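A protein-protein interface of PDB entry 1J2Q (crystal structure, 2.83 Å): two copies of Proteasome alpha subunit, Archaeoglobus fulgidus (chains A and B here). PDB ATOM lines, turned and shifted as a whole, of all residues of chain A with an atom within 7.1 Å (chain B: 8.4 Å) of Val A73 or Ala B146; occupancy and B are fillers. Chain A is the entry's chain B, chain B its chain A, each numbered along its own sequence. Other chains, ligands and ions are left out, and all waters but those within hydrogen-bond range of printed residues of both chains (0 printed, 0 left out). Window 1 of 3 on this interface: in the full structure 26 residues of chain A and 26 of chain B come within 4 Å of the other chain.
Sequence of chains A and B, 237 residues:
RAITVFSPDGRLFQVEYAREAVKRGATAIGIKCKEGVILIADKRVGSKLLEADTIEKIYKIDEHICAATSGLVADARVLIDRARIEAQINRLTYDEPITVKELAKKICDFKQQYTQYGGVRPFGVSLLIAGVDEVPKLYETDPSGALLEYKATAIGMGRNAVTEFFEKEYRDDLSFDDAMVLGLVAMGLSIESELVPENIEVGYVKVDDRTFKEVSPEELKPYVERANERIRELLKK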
ATOM      1  N   LYS A  57     -28.118 -10.344 -39.878  1.00  0.00           N
ATOM      2  CA  LYS A  57     -28.764  -9.471 -38.911  1.00  0.00           C
ATOM      3  C   LYS A  57     -30.262  -9.356 -39.108  1.00  0.00           C
ATOM      4  O   LYS A  57     -30.961  -8.821 -38.247  1.00  0.00           O
ATOM      5  CB  LYS A  57     -28.134  -8.083 -38.965  1.00  0.00           C
ATOM      6  CG  LYS A  57     -27.423  -7.678 -37.684  1.00  0.00           C
ATOM      7  CD  LYS A  57     -26.256  -8.603 -37.373  1.00  0.00           C
ATOM      8  CE  LYS A  57     -25.494  -8.127 -36.120  1.00  0.00           C
ATOM      9  NZ  LYS A  57     -24.319  -8.999 -35.755  1.00  0.00           N
ATOM     10  N   TYR A  59     -33.566 -11.667 -39.848  1.00  0.00           N
ATOM     11  CA  TYR A  59     -34.033 -13.047 -39.853  1.00  0.00           C
ATOM     12  C   TYR A  59     -35.401 -13.318 -40.463  1.00  0.00           C
ATOM     13  O   TYR A  59     -36.333 -12.508 -40.364  1.00  0.00           O
ATOM     14  CB  TYR A  59     -34.018 -13.602 -38.427  1.00  0.00           C
ATOM     15  CG  TYR A  59     -32.773 -13.237 -37.660  1.00  0.00           C
ATOM     16  CD1 TYR A  59     -32.673 -12.011 -37.008  1.00  0.00           C
ATOM     17  CD2 TYR A  59     -31.674 -14.092 -37.633  1.00  0.00           C
ATOM     18  CE1 TYR A  59     -31.513 -11.641 -36.356  1.00  0.00           C
ATOM     19  CE2 TYR A  59     -30.505 -13.734 -36.982  1.00  0.00           C
ATOM     20  CZ  TYR A  59     -30.431 -12.510 -36.350  1.00  0.00           C
ATOM     21  OH  TYR A  59     -29.263 -12.144 -35.727  1.00  0.00           O
ATOM     22  N   THR A  69     -33.173  -7.660 -34.757  1.00  0.00           N
ATOM     23  CA  THR A  69     -33.011  -7.683 -33.312  1.00  0.00           C
ATOM     24  C   THR A  69     -31.962  -6.697 -32.781  1.00  0.00           C
ATOM     25  O   THR A  69     -31.089  -6.252 -33.524  1.00  0.00           O
ATOM     26  CB  THR A  69     -32.631  -9.128 -32.862  1.00  0.00           C
ATOM     27  OG1 THR A  69     -32.571  -9.190 -31.428  1.00  0.00           O
ATOM     28  CG2 THR A  69     -31.268  -9.545 -33.432  1.00  0.00           C
ATOM     29  N   SER A  70     -32.060  -6.343 -31.500  1.00  0.00           N
ATOM     30  CA  SER A  70     -31.062  -5.461 -30.865  1.00  0.00           C
ATOM     31  C   SER A  70     -31.017  -5.692 -29.360  1.00  0.00           C
ATOM     32  O   SER A  70     -32.065  -5.824 -28.714  1.00  0.00           O
ATOM     33  CB  SER A  70     -31.343  -3.979 -31.137  1.00  0.00           C
ATOM     34  OG  SER A  70     -30.258  -3.179 -30.679  1.00  0.00           O
ATOM     35  N   GLY A  71     -29.801  -5.731 -28.812  1.00  0.00           N
ATOM     36  CA  GLY A  71     -29.612  -5.981 -27.391  1.00  0.00           C
ATOM     37  C   GLY A  71     -28.730  -7.211 -27.218  1.00  0.00           C
ATOM     38  O   GLY A  71     -27.906  -7.490 -28.098  1.00  0.00           O
ATOM     39  N   LEU A  72     -28.880  -7.943 -26.110  1.00  0.00           N
ATOM     40  CA  LEU A  72     -28.069  -9.137 -25.915  1.00  0.00           C
ATOM     41  C   LEU A  72     -28.250 -10.079 -27.107  1.00  0.00           C
ATOM     42  O   LEU A  72     -29.345 -10.573 -27.377  1.00  0.00           O
ATOM     43  CB  LEU A  72     -28.436  -9.855 -24.617  1.00  0.00           C
ATOM     44  CG  LEU A  72     -27.984  -9.178 -23.323  1.00  0.00           C
ATOM     45  CD1 LEU A  72     -26.512  -8.788 -23.429  1.00  0.00           C
ATOM     46  CD2 LEU A  72     -28.846  -7.966 -23.073  1.00  0.00           C
ATOM     47  N   VAL A  73     -27.151 -10.318 -27.813  1.00  0.00           N
ATOM     48  CA  VAL A  73     -27.134 -11.162 -28.991  1.00  0.00           C
ATOM     49  C   VAL A  73     -27.603 -12.615 -28.745  1.00  0.00           C
ATOM     50  O   VAL A  73     -28.366 -13.144 -29.543  1.00  0.00           O
ATOM     51  CB  VAL A  73     -25.712 -11.140 -29.627  1.00  0.00           C
ATOM     52  CG1 VAL A  73     -24.828 -12.193 -29.002  1.00  0.00           C
ATOM     53  CG2 VAL A  73     -25.806 -11.321 -31.107  1.00  0.00           C
ATOM     54  N   ALA A  74     -27.169 -13.251 -27.652  1.00  0.00           N
ATOM     55  CA  ALA A  74     -27.574 -14.628 -27.359  1.00  0.00           C
ATOM     56  C   ALA A  74     -29.073 -14.715 -27.066  1.00  0.00           C
ATOM     57  O   ALA A  74     -29.755 -15.613 -27.570  1.00  0.00           O
ATOM     58  CB  ALA A  74     -26.774 -15.178 -26.184  1.00  0.00           C
ATOM     59  N   ASP A  75     -29.577 -13.794 -26.244  1.00  0.00           N
ATOM     60  CA  ASP A  75     -30.994 -13.757 -25.918  1.00  0.00           C
ATOM     61  C   ASP A  75     -31.785 -13.637 -27.223  1.00  0.00           C
ATOM     62  O   ASP A  75     -32.760 -14.359 -27.451  1.00  0.00           O
ATOM     63  CB  ASP A  75     -31.328 -12.546 -25.027  1.00  0.00           C
ATOM     64  CG  ASP A  75     -30.856 -12.711 -23.600  1.00  0.00           C
ATOM     65  OD1 ASP A  75     -31.230 -11.866 -22.744  1.00  0.00           O
ATOM     66  OD2 ASP A  75     -30.116 -13.679 -23.335  1.00  0.00           O
ATOM     67  N   ALA A  76     -31.369 -12.713 -28.074  1.00  0.00           N
ATOM     68  CA  ALA A  76     -32.054 -12.504 -29.334  1.00  0.00           C
ATOM     69  C   ALA A  76     -32.265 -13.810 -30.102  1.00  0.00           C
ATOM     70  O   ALA A  76     -33.357 -14.054 -30.624  1.00  0.00           O
ATOM     71  CB  ALA A  76     -31.273 -11.532 -30.181  1.00  0.00           C
ATOM     72  N   ARG A  77     -31.220 -14.635 -30.174  1.00  0.00           N
ATOM     73  CA  ARG A  77     -31.287 -15.915 -30.873  1.00  0.00           C
ATOM     74  C   ARG A  77     -32.485 -16.735 -30.397  1.00  0.00           C
ATOM     75  O   ARG A  77     -33.379 -17.067 -31.180  1.00  0.00           O
ATOM     76  CB  ARG A  77     -30.008 -16.733 -30.650  1.00  0.00           C
ATOM     77  CG  ARG A  77     -29.092 -16.847 -31.870  1.00  0.00           C
ATOM     78  CD  ARG A  77     -28.472 -18.264 -32.010  1.00  0.00           C
ATOM     79  NE  ARG A  77     -28.093 -18.847 -30.721  1.00  0.00           N
ATOM     80  CZ  ARG A  77     -27.151 -18.363 -29.912  1.00  0.00           C
ATOM     81  NH1 ARG A  77     -26.466 -17.278 -30.253  1.00  0.00           N
ATOM     82  NH2 ARG A  77     -26.899 -18.964 -28.751  1.00  0.00           N
ATOM     83  N   VAL A  78     -32.522 -17.043 -29.108  1.00  0.00           N
ATOM     84  CA  VAL A  78     -33.611 -17.848 -28.595  1.00  0.00           C
ATOM     85  C   VAL A  78     -34.940 -17.185 -28.900  1.00  0.00           C
ATOM     86  O   VAL A  78     -35.926 -17.868 -29.190  1.00  0.00           O
ATOM     87  CB  VAL A  78     -33.467 -18.122 -27.059  1.00  0.00           C
ATOM     88  CG1 VAL A  78     -31.991 -18.081 -26.662  1.00  0.00           C
ATOM     89  CG2 VAL A  78     -34.288 -17.139 -26.241  1.00  0.00           C
ATOM     90  N   GLY A 124     -32.710  -9.180 -22.596  1.00  0.00           N
ATOM     91  CA  GLY A 124     -32.113  -7.897 -22.897  1.00  0.00           C
ATOM     92  C   GLY A 124     -32.126  -7.667 -24.390  1.00  0.00           C
ATOM     93  O   GLY A 124     -31.072  -7.467 -25.009  1.00  0.00           O
ATOM     94  N   VAL A 125     -33.315  -7.693 -24.979  1.00  0.00           N
ATOM     95  CA  VAL A 125     -33.422  -7.498 -26.410  1.00  0.00           C
ATOM     96  C   VAL A 125     -34.732  -6.863 -26.867  1.00  0.00           C
ATOM     97  O   VAL A 125     -35.776  -6.994 -26.224  1.00  0.00           O
ATOM     98  CB  VAL A 125     -33.177  -8.847 -27.158  1.00  0.00           C
ATOM     99  CG1 VAL A 125     -33.553  -9.988 -26.270  1.00  0.00           C
ATOM    100  CG2 VAL A 125     -33.998  -8.927 -28.456  1.00  0.00           C
ATOM    101  N   VAL B  15     -21.753 -13.193 -16.481  1.00  0.00           N
ATOM    102  CA  VAL B  15     -21.260 -13.515 -17.804  1.00  0.00           C
ATOM    103  C   VAL B  15     -19.911 -12.859 -18.021  1.00  0.00           C
ATOM    104  O   VAL B  15     -18.999 -13.451 -18.581  1.00  0.00           O
ATOM    105  CB  VAL B  15     -22.229 -13.029 -18.892  1.00  0.00           C
ATOM    106  CG1 VAL B  15     -21.610 -13.240 -20.267  1.00  0.00           C
ATOM    107  CG2 VAL B  15     -23.549 -13.774 -18.778  1.00  0.00           C
ATOM    108  N   ARG B  19     -16.171 -14.457 -18.466  1.00  0.00           N
ATOM    109  CA  ARG B  19     -15.237 -14.089 -19.513  1.00  0.00           C
ATOM    110  C   ARG B  19     -13.841 -13.891 -18.929  1.00  0.00           C
ATOM    111  O   ARG B  19     -12.846 -14.220 -19.563  1.00  0.00           O
ATOM    112  CB  ARG B  19     -15.721 -12.831 -20.245  1.00  0.00           C
ATOM    113  CG  ARG B  19     -16.800 -13.128 -21.285  1.00  0.00           C
ATOM    114  CD  ARG B  19     -16.892 -12.040 -22.350  1.00  0.00           C
ATOM    115  NE  ARG B  19     -17.763 -10.938 -21.970  1.00  0.00           N
ATOM    116  CZ  ARG B  19     -19.025 -10.817 -22.371  1.00  0.00           C
ATOM    117  NH1 ARG B  19     -19.551 -11.730 -23.172  1.00  0.00           N
ATOM    118  NH2 ARG B  19     -19.771  -9.793 -21.952  1.00  0.00           N
ATOM    119  N   ALA B 104     -22.740 -25.223 -33.746  1.00  0.00           N
ATOM    120  CA  ALA B 104     -22.344 -24.039 -32.983  1.00  0.00           C
ATOM    121  C   ALA B 104     -23.547 -23.342 -32.354  1.00  0.00           C
ATOM    122  O   ALA B 104     -23.536 -23.033 -31.163  1.00  0.00           O
ATOM    123  CB  ALA B 104     -21.589 -23.070 -33.889  1.00  0.00           C
ATOM    124  N   LYS B 105     -24.578 -23.092 -33.156  1.00  0.00           N
ATOM    125  CA  LYS B 105     -25.779 -22.450 -32.652  1.00  0.00           C
ATOM    126  C   LYS B 105     -26.354 -23.255 -31.491  1.00  0.00           C
ATOM    127  O   LYS B 105     -26.805 -22.697 -30.493  1.00  0.00           O
ATOM    128  CB  LYS B 105     -26.827 -22.343 -33.749  1.00  0.00           C
ATOM    129  CG  LYS B 105     -26.489 -21.366 -34.842  1.00  0.00           C
ATOM    130  CD  LYS B 105     -27.669 -21.225 -35.777  1.00  0.00           C
ATOM    131  CE  LYS B 105     -27.337 -20.399 -37.009  1.00  0.00           C
ATOM    132  NZ  LYS B 105     -28.338 -20.643 -38.113  1.00  0.00           N
ATOM    133  N   ILE B 107     -24.806 -25.455 -29.213  1.00  0.00           N
ATOM    134  CA  ILE B 107     -24.134 -25.343 -27.918  1.00  0.00           C
ATOM    135  C   ILE B 107     -24.236 -23.907 -27.408  1.00  0.00           C
ATOM    136  O   ILE B 107     -24.222 -23.658 -26.205  1.00  0.00           O
ATOM    137  CB  ILE B 107     -22.650 -25.745 -27.951  1.00  0.00           C
ATOM    138  CG1 ILE B 107     -21.992 -25.206 -29.206  1.00  0.00           C
ATOM    139  CG2 ILE B 107     -22.516 -27.249 -27.843  1.00  0.00           C
ATOM    140  CD1 ILE B 107     -20.523 -25.514 -29.252  1.00  0.00           C
ATOM    141  N   CYS B 108     -24.361 -22.955 -28.320  1.00  0.00           N
ATOM    142  CA  CYS B 108     -24.474 -21.584 -27.882  1.00  0.00           C
ATOM    143  C   CYS B 108     -25.821 -21.357 -27.208  1.00  0.00           C
ATOM    144  O   CYS B 108     -25.927 -20.568 -26.274  1.00  0.00           O
ATOM    145  CB  CYS B 108     -24.278 -20.636 -29.064  1.00  0.00           C
ATOM    146  SG  CYS B 108     -22.531 -20.427 -29.492  1.00  0.00           S
ATOM    147  N   ASP B 109     -26.851 -22.050 -27.684  1.00  0.00           N
ATOM    148  CA  ASP B 109     -28.177 -21.936 -27.094  1.00  0.00           C
ATOM    149  C   ASP B 109     -28.102 -22.626 -25.760  1.00  0.00           C
ATOM    150  O   ASP B 109     -28.716 -22.199 -24.784  1.00  0.00           O
ATOM    151  CB  ASP B 109     -29.223 -22.631 -27.950  1.00  0.00           C
ATOM    152  CG  ASP B 109     -29.619 -21.816 -29.150  1.00  0.00           C
ATOM    153  OD1 ASP B 109     -29.349 -20.597 -29.132  1.00  0.00           O
ATOM    154  OD2 ASP B 109     -30.212 -22.380 -30.103  1.00  0.00           O
ATOM    155  N   LYS B 111     -25.451 -22.891 -23.783  1.00  0.00           N
ATOM    156  CA  LYS B 111     -24.758 -21.978 -22.874  1.00  0.00           C
ATOM    157  C   LYS B 111     -25.598 -20.766 -22.493  1.00  0.00           C
ATOM    158  O   LYS B 111     -25.500 -20.260 -21.374  1.00  0.00           O
ATOM    159  CB  LYS B 111     -23.442 -21.511 -23.508  1.00  0.00           C
ATOM    160  CG  LYS B 111     -22.430 -22.639 -23.711  1.00  0.00           C
ATOM    161  CD  LYS B 111     -21.393 -22.324 -24.785  1.00  0.00           C
ATOM    162  CE  LYS B 111     -20.452 -21.204 -24.362  1.00  0.00           C
ATOM    163  NZ  LYS B 111     -19.378 -20.972 -25.357  1.00  0.00           N
ATOM    164  N   GLN B 112     -26.428 -20.309 -23.421  1.00  0.00           N
ATOM    165  CA  GLN B 112     -27.244 -19.144 -23.164  1.00  0.00           C
ATOM    166  C   GLN B 112     -28.203 -19.315 -22.006  1.00  0.00           C
ATOM    167  O   GLN B 112     -28.490 -18.359 -21.302  1.00  0.00           O
ATOM    168  CB  GLN B 112     -28.014 -18.758 -24.427  1.00  0.00           C
ATOM    169  CG  GLN B 112     -28.778 -17.439 -24.320  1.00  0.00           C
ATOM    170  CD  GLN B 112     -30.111 -17.599 -23.640  1.00  0.00           C
ATOM    171  OE1 GLN B 112     -30.733 -16.617 -23.217  1.00  0.00           O
ATOM    172  NE2 GLN B 112     -30.576 -18.846 -23.544  1.00  0.00           N
ATOM    173  N   THR B 115     -27.361 -18.693 -18.524  1.00  0.00           N
ATOM    174  CA  THR B 115     -27.195 -17.252 -18.441  1.00  0.00           C
ATOM    175  C   THR B 115     -28.429 -16.529 -17.929  1.00  0.00           C
ATOM    176  O   THR B 115     -28.335 -15.372 -17.542  1.00  0.00           O
ATOM    177  CB  THR B 115     -26.785 -16.714 -19.821  1.00  0.00           C
ATOM    178  OG1 THR B 115     -25.400 -16.379 -19.777  1.00  0.00           O
ATOM    179  CG2 THR B 115     -27.628 -15.524 -20.250  1.00  0.00           C
ATOM    180  N   VAL B 125     -16.251 -20.761 -20.092  1.00  0.00           N
ATOM    181  CA  VAL B 125     -15.496 -21.244 -21.234  1.00  0.00           C
ATOM    182  C   VAL B 125     -15.921 -20.681 -22.588  1.00  0.00           C
ATOM    183  O   VAL B 125     -17.074 -20.304 -22.811  1.00  0.00           O
ATOM    184  CB  VAL B 125     -15.517 -22.798 -21.256  1.00  0.00           C
ATOM    185  CG1 VAL B 125     -16.749 -23.289 -20.564  1.00  0.00           C
ATOM    186  CG2 VAL B 125     -15.486 -23.336 -22.684  1.00  0.00           C
ATOM    187  N   SER B 126     -14.945 -20.610 -23.486  1.00  0.00           N
ATOM    188  CA  SER B 126     -15.141 -20.102 -24.837  1.00  0.00           C
ATOM    189  C   SER B 126     -14.687 -21.197 -25.792  1.00  0.00           C
ATOM    190  O   SER B 126     -13.726 -21.927 -25.512  1.00  0.00           O
ATOM    191  CB  SER B 126     -14.307 -18.839 -25.034  1.00  0.00           C
ATOM    192  OG  SER B 126     -14.637 -18.194 -26.242  1.00  0.00           O
ATOM    193  N   LEU B 127     -15.372 -21.321 -26.920  1.00  0.00           N
ATOM    194  CA  LEU B 127     -15.025 -22.381 -27.862  1.00  0.00           C
ATOM    195  C   LEU B 127     -14.683 -21.982 -29.271  1.00  0.00           C
ATOM    196  O   LEU B 127     -15.244 -21.033 -29.827  1.00  0.00           O
ATOM    197  CB  LEU B 127     -16.162 -23.389 -27.988  1.00  0.00           C
ATOM    198  CG  LEU B 127     -16.657 -24.164 -26.784  1.00  0.00           C
ATOM    199  CD1 LEU B 127     -17.964 -24.843 -27.157  1.00  0.00           C
ATOM    200  CD2 LEU B 127     -15.601 -25.167 -26.355  1.00  0.00           C
ATOM    201  N   TYR B 139     -15.920 -20.919 -36.099  1.00  0.00           N
ATOM    202  CA  TYR B 139     -16.783 -20.173 -35.201  1.00  0.00           C
ATOM    203  C   TYR B 139     -16.138 -20.137 -33.827  1.00  0.00           C
ATOM    204  O   TYR B 139     -15.386 -21.042 -33.453  1.00  0.00           O
ATOM    205  CB  TYR B 139     -18.148 -20.856 -35.105  1.00  0.00           C
ATOM    206  CG  TYR B 139     -18.970 -20.780 -36.365  1.00  0.00           C
ATOM    207  CD1 TYR B 139     -19.763 -19.666 -36.641  1.00  0.00           C
ATOM    208  CD2 TYR B 139     -18.946 -21.814 -37.295  1.00  0.00           C
ATOM    209  CE1 TYR B 139     -20.513 -19.585 -37.821  1.00  0.00           C
ATOM    210  CE2 TYR B 139     -19.688 -21.744 -38.473  1.00  0.00           C
ATOM    211  CZ  TYR B 139     -20.463 -20.627 -38.729  1.00  0.00           C
ATOM    212  OH  TYR B 139     -21.159 -20.536 -39.911  1.00  0.00           O
ATOM    213  N   GLU B 140     -16.414 -19.077 -33.085  1.00  0.00           N
ATOM    214  CA  GLU B 140     -15.886 -18.966 -31.742  1.00  0.00           C
ATOM    215  C   GLU B 140     -17.088 -18.595 -30.884  1.00  0.00           C
ATOM    216  O   GLU B 140     -17.936 -17.796 -31.296  1.00  0.00           O
ATOM    217  CB  GLU B 140     -14.801 -17.895 -31.681  1.00  0.00           C
ATOM    218  CG  GLU B 140     -15.332 -16.489 -31.570  1.00  0.00           C
ATOM    219  CD  GLU B 140     -15.375 -16.031 -30.143  1.00  0.00           C
ATOM    220  OE1 GLU B 140     -16.145 -15.088 -29.850  1.00  0.00           O
ATOM    221  OE2 GLU B 140     -14.627 -16.617 -29.326  1.00  0.00           O
ATOM    222  N   THR B 141     -17.175 -19.201 -29.704  1.00  0.00           N
ATOM    223  CA  THR B 141     -18.301 -18.957 -28.806  1.00  0.00           C
ATOM    224  C   THR B 141     -17.896 -18.198 -27.558  1.00  0.00           C
ATOM    225  O   THR B 141     -16.734 -18.171 -27.175  1.00  0.00           O
ATOM    226  CB  THR B 141     -18.956 -20.279 -28.372  1.00  0.00           C
ATOM    227  OG1 THR B 141     -17.991 -21.083 -27.678  1.00  0.00           O
ATOM    228  CG2 THR B 141     -19.467 -21.039 -29.581  1.00  0.00           C
ATOM    229  N   ASP B 142     -18.885 -17.611 -26.907  1.00  0.00           N
ATOM    230  CA  ASP B 142     -18.667 -16.828 -25.709  1.00  0.00           C
ATOM    231  C   ASP B 142     -19.498 -17.372 -24.547  1.00  0.00           C
ATOM    232  O   ASP B 142     -20.533 -18.010 -24.746  1.00  0.00           O
ATOM    233  CB  ASP B 142     -19.075 -15.394 -26.028  1.00  0.00           C
ATOM    234  CG  ASP B 142     -18.946 -14.473 -24.857  1.00  0.00           C
ATOM    235  OD1 ASP B 142     -17.800 -14.182 -24.446  1.00  0.00           O
ATOM    236  OD2 ASP B 142     -20.005 -14.036 -24.352  1.00  0.00           O
ATOM    237  N   PRO B 143     -19.047 -17.142 -23.312  1.00  0.00           N
ATOM    238  CA  PRO B 143     -19.781 -17.614 -22.133  1.00  0.00           C
ATOM    239  C   PRO B 143     -21.253 -17.199 -22.126  1.00  0.00           C
ATOM    240  O   PRO B 143     -22.075 -17.832 -21.479  1.00  0.00           O
ATOM    241  CB  PRO B 143     -19.005 -16.982 -20.980  1.00  0.00           C
ATOM    242  CG  PRO B 143     -17.587 -17.077 -21.480  1.00  0.00           C
ATOM    243  CD  PRO B 143     -17.706 -16.655 -22.937  1.00  0.00           C
ATOM    244  N   SER B 144     -21.581 -16.134 -22.842  1.00  0.00           N
ATOM    245  CA  SER B 144     -22.958 -15.648 -22.900  1.00  0.00           C
ATOM    246  C   SER B 144     -23.810 -16.428 -23.893  1.00  0.00           C
ATOM    247  O   SER B 144     -25.039 -16.370 -23.845  1.00  0.00           O
ATOM    248  CB  SER B 144     -22.988 -14.183 -23.318  1.00  0.00           C
ATOM    249  OG  SER B 144     -22.680 -14.068 -24.693  1.00  0.00           O
ATOM    250  N   GLY B 145     -23.154 -17.137 -24.802  1.00  0.00           N
ATOM    251  CA  GLY B 145     -23.878 -17.894 -25.806  1.00  0.00           C
ATOM    252  C   GLY B 145     -23.864 -17.162 -27.137  1.00  0.00           C
ATOM    253  O   GLY B 145     -24.614 -17.500 -28.059  1.00  0.00           O
ATOM    254  N   ALA B 146     -23.006 -16.148 -27.237  1.00  0.00           N
ATOM    255  CA  ALA B 146     -22.885 -15.371 -28.463  1.00  0.00           C
ATOM    256  C   ALA B 146     -22.004 -16.159 -29.431  1.00  0.00           C
ATOM    257  O   ALA B 146     -21.020 -16.783 -29.028  1.00  0.00           O
ATOM    258  CB  ALA B 146     -22.280 -14.017 -28.164  1.00  0.00           C
ATOM    259  N   LEU B 147     -22.364 -16.123 -30.706  1.00  0.00           N
ATOM    260  CA  LEU B 147     -21.643 -16.856 -31.735  1.00  0.00           C
ATOM    261  C   LEU B 147     -21.049 -15.880 -32.746  1.00  0.00           C
ATOM    262  O   LEU B 147     -21.652 -14.847 -33.042  1.00  0.00           O
ATOM    263  CB  LEU B 147     -22.623 -17.783 -32.453  1.00  0.00           C
ATOM    264  CG  LEU B 147     -22.204 -19.172 -32.901  1.00  0.00           C
ATOM    265  CD1 LEU B 147     -23.180 -19.620 -33.964  1.00  0.00           C
ATOM    266  CD2 LEU B 147     -20.815 -19.176 -33.461  1.00  0.00           C
ATOM    267  N   LEU B 148     -19.882 -16.214 -33.284  1.00  0.00           N
ATOM    268  CA  LEU B 148     -19.232 -15.377 -34.282  1.00  0.00           C
ATOM    269  C   LEU B 148     -18.420 -16.209 -35.263  1.00  0.00           C
ATOM    270  O   LEU B 148     -17.705 -17.130 -34.860  1.00  0.00           O
ATOM    271  CB  LEU B 148     -18.308 -14.349 -33.610  1.00  0.00           C
ATOM    272  CG  LEU B 148     -18.933 -13.090 -33.008  1.00  0.00           C
ATOM    273  CD1 LEU B 148     -17.857 -12.224 -32.410  1.00  0.00           C
ATOM    274  CD2 LEU B 148     -19.679 -12.332 -34.067  1.00  0.00           C
ATOM    275  N   GLU B 149     -18.530 -15.888 -36.551  1.00  0.00           N
ATOM    276  CA  GLU B 149     -17.763 -16.607 -37.562  1.00  0.00           C
ATOM    277  C   GLU B 149     -16.544 -15.785 -37.959  1.00  0.00           C
ATOM    278  O   GLU B 149     -16.666 -14.645 -38.384  1.00  0.00           O
ATOM    279  CB  GLU B 149     -18.597 -16.892 -38.795  1.00  0.00           C
ATOM    280  CG  GLU B 149     -17.874 -17.791 -39.770  1.00  0.00           C
ATOM    281  CD  GLU B 149     -18.652 -17.982 -41.061  1.00  0.00           C
ATOM    282  OE1 GLU B 149     -18.166 -18.661 -41.996  1.00  0.00           O
ATOM    283  OE2 GLU B 149     -19.763 -17.441 -41.137  1.00  0.00           O
ATOM    284  N   TYR B 150     -15.371 -16.381 -37.801  1.00  0.00           N
ATOM    285  CA  TYR B 150     -14.107 -15.733 -38.119  1.00  0.00           C
ATOM    286  C   TYR B 150     -13.384 -16.379 -39.307  1.00  0.00           C
ATOM    287  O   TYR B 150     -13.639 -17.531 -39.660  1.00  0.00           O
ATOM    288  CB  TYR B 150     -13.157 -15.793 -36.908  1.00  0.00           C
ATOM    289  CG  TYR B 150     -13.481 -14.842 -35.785  1.00  0.00           C
ATOM    290  CD1 TYR B 150     -14.521 -15.105 -34.901  1.00  0.00           C
ATOM    291  CD2 TYR B 150     -12.723 -13.690 -35.589  1.00  0.00           C
ATOM    292  CE1 TYR B 150     -14.798 -14.244 -33.839  1.00  0.00           C
ATOM    293  CE2 TYR B 150     -12.989 -12.822 -34.536  1.00  0.00           C
ATOM    294  CZ  TYR B 150     -14.023 -13.103 -33.660  1.00  0.00           C
ATOM    295  OH  TYR B 150     -14.265 -12.248 -32.601  1.00  0.00           O
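The backbone carbonyl oxygen (O) of Cys B108 sits close to the guanidinium group (NH2) of Arg A77, 3.1 Å away.
The side-chain amide oxygen of Gln B112 sits close to the side-chain carboxylate of Asp A75 (3.0 Å).
O of Gly B145 is in hydrogen-bond range of NH2 of Arg A77, 2.8 Å away.
OD1 of Asp B109 is in salt-bridge range of NE of Arg A77 (2.7 Å).
The backbone NH (N) of Ala B146 sits at hydrogen-bond distance from the side-chain hydroxyl (OG) of Ser B144, at 3.3 Å.
The side-chain carboxylate (OD2) of Asp B142 lies within hydrogen-bond range of the side-chain hydroxyl (OG) of Ser B144 (2.7 Å).
N of Gly A124 is in hydrogen-bond range of OD1 of Asp A75, 3.1 Å away.
The side-chain sulfur of Cys B108 lies within hydrogen-bond range of the backbone carbonyl oxygen of Ala B104, at 3.3 Å.
Among the printed residues, pairs that only touch across the chains: Ala A74 with Ser B144 (3.1 Å), Val A73 with Ala B146 (3.2 Å), Val A78 with Gln B112 (3.5 Å), Ala A74 with Gln B112 (3.6 Å) and Ala A74 with Gly B145 (3.6 Å).
Val A73 touches just one residue of chain B: Ala B146 (3.2 Å).
Of chain B, only Gln B112, Ser B144 and Gly B145 come within 4 Å of Ala A74.
Of the printed residues of chain A, Gln B112 touches Ala A74, Asp A75 and Val A78.
Of the printed residues of chain A, Ser B144 touches Ala A74 (3.1 Å).
Gly B145 touches just these residues of chain A: Ala A74 (3.6 Å) and Arg A77 (2.8 Å).
Ala B146 touches just one residue of chain A: Val A73 (3.2 Å).
Glu B149 touches none of the printed residues of chain A.
The nearest residue of chain B that does not touch Val A73 is Leu B147 (4.9 Å).
The nearest residue of chain A that does not touch Ala B146 is Ala A74 (4.03 Å).
Printed residues of chain B that touch a printed residue of chain A: Cys B108, Asp B109, Gln B112, Ser B144, Gly B145 and Ala B146.
Hydrophobic or aromatic side chains of chain B within 4 Å of the printed part of chain A: Ala B146.
Hydrophobic or aromatic side chains of chain A that line the printed part of chain B: Val A73, Ala A74 and Val A78.
Among the printed residues, Asp or Glu carboxylates within 4 Å of a Lys or Arg side-chain nitrogen of the other chain: Arg A77 with Asp B109.
Position printed for both chains: 125.
Of the 9 pairs that touch across the chains among the printed residues, none has its exchanged pair printed and touching as well.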
